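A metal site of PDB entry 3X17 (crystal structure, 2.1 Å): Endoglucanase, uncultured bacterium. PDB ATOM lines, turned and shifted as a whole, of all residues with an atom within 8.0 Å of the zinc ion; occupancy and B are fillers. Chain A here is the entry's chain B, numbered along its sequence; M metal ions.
The backbone NH (N) of Cys 132 lies within hydrogen-bond range of the backbone carbonyl oxygen (O) of Gly 173, at 2.9 Å.
The side-chain sulfur (SG) of Cys 132 lies close to the guanidinium group (NH2) of Arg 265, 3.6 Å away.
OD1 of Asp 148 sits at hydrogen-bond distance from NE2 of His 145.
O of Gln 130 is in hydrogen-bond range of N of His 175, at 2.7 Å.
The side-chain carboxylate (OD1) of Asp 148 is in hydrogen-bond range of the backbone NH (N) of Gly 133 (2.9 Å).
The backbone NH (N) of Val 134 is in hydrogen-bond range of the side-chain carboxylate (OD1) of Asp 148, at 3.2 Å.
A ring nitrogen (NE2) of His 149 lies within hydrogen-bond range of the side-chain carboxylate (OD2) of Asp 261.
OD2 of Asp 152 sits close to SG of Cys 132, at 3.7 Å.
N of Gly 133 touches the zinc ion (3.9 Å).
The nearest printed residue that does not touch the zinc ion is Arg 265 (4.3 Å).
The zinc ion is bound by the side-chain carboxylate of Asp 148 (1.9 Å), a ring nitrogen (NE2) of His 175 (2.1 Å), a ring nitrogen (ND1) of His 149 (2.1 Å) and the side-chain sulfur of Cys 132 (2.2 Å).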
ATOM      1  N   GLN A 130       9.269 -16.523  27.955  1.00  0.00           N
ATOM      2  CA  GLN A 130       9.890 -17.314  26.882  1.00  0.00           C
ATOM      3  C   GLN A 130       9.270 -18.701  26.702  1.00  0.00           C
ATOM      4  O   GLN A 130       9.693 -19.456  25.822  1.00  0.00           O
ATOM      5  CB  GLN A 130      11.386 -17.479  27.142  1.00  0.00           C
ATOM      6  CG  GLN A 130      12.203 -16.196  27.081  1.00  0.00           C
ATOM      7  CD  GLN A 130      12.576 -15.789  25.666  1.00  0.00           C
ATOM      8  OE1 GLN A 130      12.142 -14.762  25.173  1.00  0.00           O
ATOM      9  NE2 GLN A 130      13.329 -16.646  24.991  1.00  0.00           N
ATOM     10  N   ARG A 131       8.353 -19.089  27.580  1.00  0.00           N
ATOM     11  CA  ARG A 131       7.761 -20.430  27.503  1.00  0.00           C
ATOM     12  C   ARG A 131       7.125 -20.741  26.156  1.00  0.00           C
ATOM     13  O   ARG A 131       6.581 -19.852  25.495  1.00  0.00           O
ATOM     14  CB  ARG A 131       6.724 -20.648  28.591  1.00  0.00           C
ATOM     15  CG  ARG A 131       7.289 -20.740  30.011  1.00  0.00           C
ATOM     16  CD  ARG A 131       6.150 -20.985  31.061  1.00  0.00           C
ATOM     17  NE  ARG A 131       6.650 -20.911  32.440  1.00  0.00           N
ATOM     18  CZ  ARG A 131       5.918 -21.176  33.526  1.00  0.00           C
ATOM     19  NH1 ARG A 131       4.638 -21.526  33.412  1.00  0.00           N
ATOM     20  NH2 ARG A 131       6.470 -21.114  34.745  1.00  0.00           N
ATOM     21  N   CYS A 132       7.268 -21.983  25.706  1.00  0.00           N
ATOM     22  CA  CYS A 132       6.783 -22.421  24.404  1.00  0.00           C
ATOM     23  C   CYS A 132       5.642 -23.397  24.657  1.00  0.00           C
ATOM     24  O   CYS A 132       5.643 -24.092  25.678  1.00  0.00           O
ATOM     25  CB  CYS A 132       7.904 -23.158  23.675  1.00  0.00           C
ATOM     26  SG  CYS A 132       7.550 -23.803  22.006  1.00  0.00           S
ATOM     27  N   GLY A 133       4.641 -23.377  23.786  1.00  0.00           N
ATOM     28  CA  GLY A 133       3.619 -24.398  23.843  1.00  0.00           C
ATOM     29  C   GLY A 133       2.455 -24.020  24.748  1.00  0.00           C
ATOM     30  O   GLY A 133       1.712 -24.883  25.219  1.00  0.00           O
ATOM     31  N   VAL A 134       2.325 -22.744  25.058  1.00  0.00           N
ATOM     32  CA  VAL A 134       1.277 -22.335  25.969  1.00  0.00           C
ATOM     33  C   VAL A 134       0.908 -20.890  25.674  1.00  0.00           C
ATOM     34  O   VAL A 134       1.790 -20.079  25.371  1.00  0.00           O
ATOM     35  CB  VAL A 134       1.718 -22.475  27.442  1.00  0.00           C
ATOM     36  CG1 VAL A 134       2.966 -21.577  27.736  1.00  0.00           C
ATOM     37  CG2 VAL A 134       0.540 -22.141  28.376  1.00  0.00           C
ATOM     38  N   HIS A 145       0.555 -13.977  23.225  1.00  0.00           N
ATOM     39  CA  HIS A 145       0.489 -14.734  21.992  1.00  0.00           C
ATOM     40  C   HIS A 145      -0.364 -15.946  22.267  1.00  0.00           C
ATOM     41  O   HIS A 145      -0.440 -16.396  23.409  1.00  0.00           O
ATOM     42  CB  HIS A 145       1.897 -15.123  21.510  1.00  0.00           C
ATOM     43  CG  HIS A 145       2.591 -16.149  22.371  1.00  0.00           C
ATOM     44  ND1 HIS A 145       3.725 -15.860  23.106  1.00  0.00           N
ATOM     45  CD2 HIS A 145       2.354 -17.477  22.528  1.00  0.00           C
ATOM     46  CE1 HIS A 145       4.142 -16.965  23.712  1.00  0.00           C
ATOM     47  NE2 HIS A 145       3.313 -17.959  23.397  1.00  0.00           N
ATOM     48  N   ALA A 146      -1.019 -16.456  21.235  1.00  0.00           N
ATOM     49  CA  ALA A 146      -1.842 -17.662  21.378  1.00  0.00           C
ATOM     50  C   ALA A 146      -0.942 -18.882  21.456  1.00  0.00           C
ATOM     51  O   ALA A 146       0.290 -18.783  21.342  1.00  0.00           O
ATOM     52  CB  ALA A 146      -2.821 -17.799  20.183  1.00  0.00           C
ATOM     53  N   LEU A 147      -1.539 -20.054  21.580  1.00  0.00           N
ATOM     54  CA  LEU A 147      -0.836 -21.300  21.678  1.00  0.00           C
ATOM     55  C   LEU A 147       0.125 -21.492  20.537  1.00  0.00           C
ATOM     56  O   LEU A 147      -0.253 -21.420  19.410  1.00  0.00           O
ATOM     57  CB  LEU A 147      -1.822 -22.432  21.651  1.00  0.00           C
ATOM     58  CG  LEU A 147      -1.559 -23.705  22.420  1.00  0.00           C
ATOM     59  CD1 LEU A 147      -2.166 -24.880  21.766  1.00  0.00           C
ATOM     60  CD2 LEU A 147      -0.155 -23.940  22.678  1.00  0.00           C
ATOM     61  N   ASP A 148       1.369 -21.771  20.850  1.00  0.00           N
ATOM     62  CA  ASP A 148       2.401 -21.949  19.805  1.00  0.00           C
ATOM     63  C   ASP A 148       2.966 -23.352  19.810  1.00  0.00           C
ATOM     64  O   ASP A 148       3.191 -23.936  20.881  1.00  0.00           O
ATOM     65  CB  ASP A 148       3.549 -20.962  20.053  1.00  0.00           C
ATOM     66  CG  ASP A 148       4.109 -21.077  21.481  1.00  0.00           C
ATOM     67  OD1 ASP A 148       3.321 -21.106  22.449  1.00  0.00           O
ATOM     68  OD2 ASP A 148       5.353 -21.203  21.619  1.00  0.00           O
ATOM     69  N   HIS A 149       3.323 -23.853  18.637  1.00  0.00           N
ATOM     70  CA  HIS A 149       4.217 -24.994  18.566  1.00  0.00           C
ATOM     71  C   HIS A 149       3.623 -26.131  19.374  1.00  0.00           C
ATOM     72  O   HIS A 149       4.337 -26.975  19.922  1.00  0.00           O
ATOM     73  CB  HIS A 149       5.618 -24.633  19.106  1.00  0.00           C
ATOM     74  CG  HIS A 149       6.312 -23.564  18.313  1.00  0.00           C
ATOM     75  ND1 HIS A 149       6.754 -22.390  18.876  1.00  0.00           N
ATOM     76  CD2 HIS A 149       6.578 -23.475  16.984  1.00  0.00           C
ATOM     77  CE1 HIS A 149       7.298 -21.628  17.937  1.00  0.00           C
ATOM     78  NE2 HIS A 149       7.193 -22.264  16.780  1.00  0.00           N
ATOM     79  N   HIS A 150       2.300 -26.229  19.301  1.00  0.00           N
ATOM     80  CA  HIS A 150       1.610 -27.365  19.870  1.00  0.00           C
ATOM     81  C   HIS A 150       1.875 -28.696  19.138  1.00  0.00           C
ATOM     82  O   HIS A 150       1.493 -29.757  19.637  1.00  0.00           O
ATOM     83  CB  HIS A 150       0.107 -27.121  19.959  1.00  0.00           C
ATOM     84  CG  HIS A 150      -0.606 -28.083  20.850  1.00  0.00           C
ATOM     85  ND1 HIS A 150      -1.294 -29.189  20.366  1.00  0.00           N
ATOM     86  CD2 HIS A 150      -0.642 -28.186  22.203  1.00  0.00           C
ATOM     87  CE1 HIS A 150      -1.810 -29.861  21.381  1.00  0.00           C
ATOM     88  NE2 HIS A 150      -1.419 -29.282  22.509  1.00  0.00           N
ATOM     89  N   ASP A 152       4.978 -29.871  18.498  1.00  0.00           N
ATOM     90  CA  ASP A 152       6.396 -30.234  18.733  1.00  0.00           C
ATOM     91  C   ASP A 152       6.437 -31.676  19.249  1.00  0.00           C
ATOM     92  O   ASP A 152       5.823 -31.946  20.277  1.00  0.00           O
ATOM     93  CB  ASP A 152       7.020 -29.326  19.823  1.00  0.00           C
ATOM     94  CG  ASP A 152       7.322 -27.907  19.345  1.00  0.00           C
ATOM     95  OD1 ASP A 152       7.186 -27.621  18.132  1.00  0.00           O
ATOM     96  OD2 ASP A 152       7.714 -27.057  20.192  1.00  0.00           O
ATOM     97  N   THR A 171       6.302 -31.007  23.538  1.00  0.00           N
ATOM     98  CA  THR A 171       5.788 -29.683  23.660  1.00  0.00           C
ATOM     99  C   THR A 171       6.327 -29.028  24.950  1.00  0.00           C
ATOM    100  O   THR A 171       6.865 -29.691  25.748  1.00  0.00           O
ATOM    101  CB  THR A 171       4.258 -29.813  23.627  1.00  0.00           C
ATOM    102  OG1 THR A 171       3.687 -28.568  23.304  1.00  0.00           O
ATOM    103  CG2 THR A 171       3.737 -30.315  24.911  1.00  0.00           C
ATOM    104  N   GLY A 172       6.209 -27.718  25.119  1.00  0.00           N
ATOM    105  CA  GLY A 172       6.615 -27.039  26.371  1.00  0.00           C
ATOM    106  C   GLY A 172       8.061 -26.528  26.311  1.00  0.00           C
ATOM    107  O   GLY A 172       8.607 -26.367  25.217  1.00  0.00           O
ATOM    108  N   GLY A 173       8.698 -26.368  27.468  1.00  0.00           N
ATOM    109  CA  GLY A 173      10.057 -25.811  27.518  1.00  0.00           C
ATOM    110  C   GLY A 173      10.124 -24.315  27.204  1.00  0.00           C
ATOM    111  O   GLY A 173       9.090 -23.622  27.226  1.00  0.00           O
ATOM    112  N   TRP A 174      11.342 -23.819  26.997  1.00  0.00           N
ATOM    113  CA  TRP A 174      11.566 -22.379  26.731  1.00  0.00           C
ATOM    114  C   TRP A 174      12.030 -22.131  25.306  1.00  0.00           C
ATOM    115  O   TRP A 174      12.992 -22.775  24.861  1.00  0.00           O
ATOM    116  CB  TRP A 174      12.668 -21.830  27.660  1.00  0.00           C
ATOM    117  CG  TRP A 174      12.379 -21.941  29.147  1.00  0.00           C
ATOM    118  CD1 TRP A 174      11.274 -21.477  29.804  1.00  0.00           C
ATOM    119  CD2 TRP A 174      13.210 -22.575  30.136  1.00  0.00           C
ATOM    120  NE1 TRP A 174      11.369 -21.788  31.155  1.00  0.00           N
ATOM    121  CE2 TRP A 174      12.557 -22.444  31.382  1.00  0.00           C
ATOM    122  CE3 TRP A 174      14.463 -23.205  30.098  1.00  0.00           C
ATOM    123  CZ2 TRP A 174      13.117 -22.911  32.583  1.00  0.00           C
ATOM    124  CZ3 TRP A 174      15.024 -23.666  31.306  1.00  0.00           C
ATOM    125  CH2 TRP A 174      14.335 -23.527  32.526  1.00  0.00           C
ATOM    126  N   HIS A 175      11.459 -21.127  24.643  1.00  0.00           N
ATOM    127  CA  HIS A 175      12.135 -20.540  23.484  1.00  0.00           C
ATOM    128  C   HIS A 175      13.541 -20.127  23.896  1.00  0.00           C
ATOM    129  O   HIS A 175      13.716 -19.530  24.967  1.00  0.00           O
ATOM    130  CB  HIS A 175      11.379 -19.327  22.939  1.00  0.00           C
ATOM    131  CG  HIS A 175      10.019 -19.648  22.424  1.00  0.00           C
ATOM    132  ND1 HIS A 175       8.954 -18.774  22.534  1.00  0.00           N
ATOM    133  CD2 HIS A 175       9.515 -20.769  21.852  1.00  0.00           C
ATOM    134  CE1 HIS A 175       7.881 -19.319  22.002  1.00  0.00           C
ATOM    135  NE2 HIS A 175       8.194 -20.532  21.576  1.00  0.00           N
ATOM    136  N   ASP A 179      14.992 -16.715  18.672  1.00  0.00           N
ATOM    137  CA  ASP A 179      14.257 -17.674  17.863  1.00  0.00           C
ATOM    138  C   ASP A 179      13.352 -18.483  18.762  1.00  0.00           C
ATOM    139  O   ASP A 179      13.143 -18.152  19.952  1.00  0.00           O
ATOM    140  CB  ASP A 179      15.225 -18.617  17.130  1.00  0.00           C
ATOM    141  CG  ASP A 179      16.056 -19.452  18.081  1.00  0.00           C
ATOM    142  OD1 ASP A 179      16.497 -18.890  19.107  1.00  0.00           O
ATOM    143  OD2 ASP A 179      16.241 -20.660  17.837  1.00  0.00           O
ATOM    144  N   TYR A 180      12.812 -19.559  18.197  1.00  0.00           N
ATOM    145  CA  TYR A 180      11.840 -20.382  18.919  1.00  0.00           C
ATOM    146  C   TYR A 180      12.302 -21.820  19.042  1.00  0.00           C
ATOM    147  O   TYR A 180      11.574 -22.676  19.585  1.00  0.00           O
ATOM    148  CB  TYR A 180      10.457 -20.332  18.227  1.00  0.00           C
ATOM    149  CG  TYR A 180       9.865 -18.946  18.132  1.00  0.00           C
ATOM    150  CD1 TYR A 180       9.836 -18.101  19.238  1.00  0.00           C
ATOM    151  CD2 TYR A 180       9.294 -18.490  16.944  1.00  0.00           C
ATOM    152  CE1 TYR A 180       9.296 -16.821  19.160  1.00  0.00           C
ATOM    153  CE2 TYR A 180       8.705 -17.223  16.874  1.00  0.00           C
ATOM    154  CZ  TYR A 180       8.718 -16.394  17.972  1.00  0.00           C
ATOM    155  OH  TYR A 180       8.179 -15.107  17.901  1.00  0.00           O
ATOM    156  N   GLY A 181      13.530 -22.087  18.619  1.00  0.00           N
ATOM    157  CA  GLY A 181      14.149 -23.383  18.858  1.00  0.00           C
ATOM    158  C   GLY A 181      14.273 -23.709  20.338  1.00  0.00           C
ATOM    159  O   GLY A 181      14.286 -22.818  21.178  1.00  0.00           O
ATOM    160  N   LYS A 182      14.232 -24.993  20.675  1.00  0.00           N
ATOM    161  CA  LYS A 182      14.380 -25.420  22.052  1.00  0.00           C
ATOM    162  C   LYS A 182      15.524 -26.415  22.088  1.00  0.00           C
ATOM    163  O   LYS A 182      15.645 -27.257  21.206  1.00  0.00           O
ATOM    164  CB  LYS A 182      13.089 -26.087  22.531  1.00  0.00           C
ATOM    165  CG  LYS A 182      11.826 -25.204  22.293  1.00  0.00           C
ATOM    166  CD  LYS A 182      10.586 -25.798  22.955  1.00  0.00           C
ATOM    167  CE  LYS A 182      10.232 -27.165  22.398  1.00  0.00           C
ATOM    168  NZ  LYS A 182       8.803 -27.548  22.760  1.00  0.00           N
ATOM    169  N   ARG A 257       5.289 -13.788  15.082  1.00  0.00           N
ATOM    170  CA  ARG A 257       4.847 -14.416  16.341  1.00  0.00           C
ATOM    171  C   ARG A 257       5.042 -15.928  16.324  1.00  0.00           C
ATOM    172  O   ARG A 257       5.041 -16.544  15.251  1.00  0.00           O
ATOM    173  CB  ARG A 257       3.365 -14.138  16.599  1.00  0.00           C
ATOM    174  CG  ARG A 257       3.020 -12.685  16.819  1.00  0.00           C
ATOM    175  CD  ARG A 257       1.566 -12.387  16.405  1.00  0.00           C
ATOM    176  NE  ARG A 257       1.324 -10.947  16.361  1.00  0.00           N
ATOM    177  CZ  ARG A 257       1.233 -10.178  17.437  1.00  0.00           C
ATOM    178  NH1 ARG A 257       1.361 -10.722  18.637  1.00  0.00           N
ATOM    179  NH2 ARG A 257       1.051  -8.864  17.317  1.00  0.00           N
ATOM    180  N   PRO A 258       5.115 -16.538  17.526  1.00  0.00           N
ATOM    181  CA  PRO A 258       5.390 -17.975  17.589  1.00  0.00           C
ATOM    182  C   PRO A 258       4.223 -18.813  17.078  1.00  0.00           C
ATOM    183  O   PRO A 258       4.447 -19.926  16.593  1.00  0.00           O
ATOM    184  CB  PRO A 258       5.629 -18.230  19.079  1.00  0.00           C
ATOM    185  CG  PRO A 258       4.982 -17.126  19.785  1.00  0.00           C
ATOM    186  CD  PRO A 258       5.048 -15.920  18.852  1.00  0.00           C
ATOM    187  N   GLU A 259       2.999 -18.311  17.224  1.00  0.00           N
ATOM    188  CA  GLU A 259       1.817 -19.020  16.736  1.00  0.00           C
ATOM    189  C   GLU A 259       1.711 -18.940  15.227  1.00  0.00           C
ATOM    190  O   GLU A 259       1.008 -19.726  14.624  1.00  0.00           O
ATOM    191  CB  GLU A 259       0.517 -18.485  17.339  1.00  0.00           C
ATOM    192  CG  GLU A 259       0.643 -17.774  18.669  1.00  0.00           C
ATOM    193  CD  GLU A 259       1.086 -16.336  18.512  1.00  0.00           C
ATOM    194  OE1 GLU A 259       2.312 -16.133  18.455  1.00  0.00           O
ATOM    195  OE2 GLU A 259       0.238 -15.409  18.495  1.00  0.00           O
ATOM    196  N   ASP A 261       4.426 -19.441  13.508  1.00  0.00           N
ATOM    197  CA  ASP A 261       5.546 -20.268  13.062  1.00  0.00           C
ATOM    198  C   ASP A 261       5.052 -21.690  12.985  1.00  0.00           C
ATOM    199  O   ASP A 261       5.143 -22.456  13.944  1.00  0.00           O
ATOM    200  CB  ASP A 261       6.755 -20.164  14.014  1.00  0.00           C
ATOM    201  CG  ASP A 261       7.940 -21.011  13.560  1.00  0.00           C
ATOM    202  OD1 ASP A 261       8.258 -21.000  12.358  1.00  0.00           O
ATOM    203  OD2 ASP A 261       8.588 -21.669  14.402  1.00  0.00           O
ATOM    204  N   ARG A 265       8.008 -29.089  13.074  1.00  0.00           N
ATOM    205  CA  ARG A 265       9.213 -29.050  13.896  1.00  0.00           C
ATOM    206  C   ARG A 265       9.692 -30.449  14.238  1.00  0.00           C
ATOM    207  O   ARG A 265       8.890 -31.335  14.498  1.00  0.00           O
ATOM    208  CB  ARG A 265       8.979 -28.247  15.183  1.00  0.00           C
ATOM    209  CG  ARG A 265       8.435 -26.851  14.910  1.00  0.00           C
ATOM    210  CD  ARG A 265       9.256 -25.789  15.597  1.00  0.00           C
ATOM    211  NE  ARG A 265       9.111 -25.824  17.058  1.00  0.00           N
ATOM    212  CZ  ARG A 265       9.692 -24.922  17.851  1.00  0.00           C
ATOM    213  NH1 ARG A 265      10.422 -23.968  17.302  1.00  0.00           N
ATOM    214  NH2 ARG A 265       9.490 -24.929  19.150  1.00  0.00           N
HETATM  215 ZN    ZN M   1       6.934 -22.033  20.928  1.00  0.00          ZN
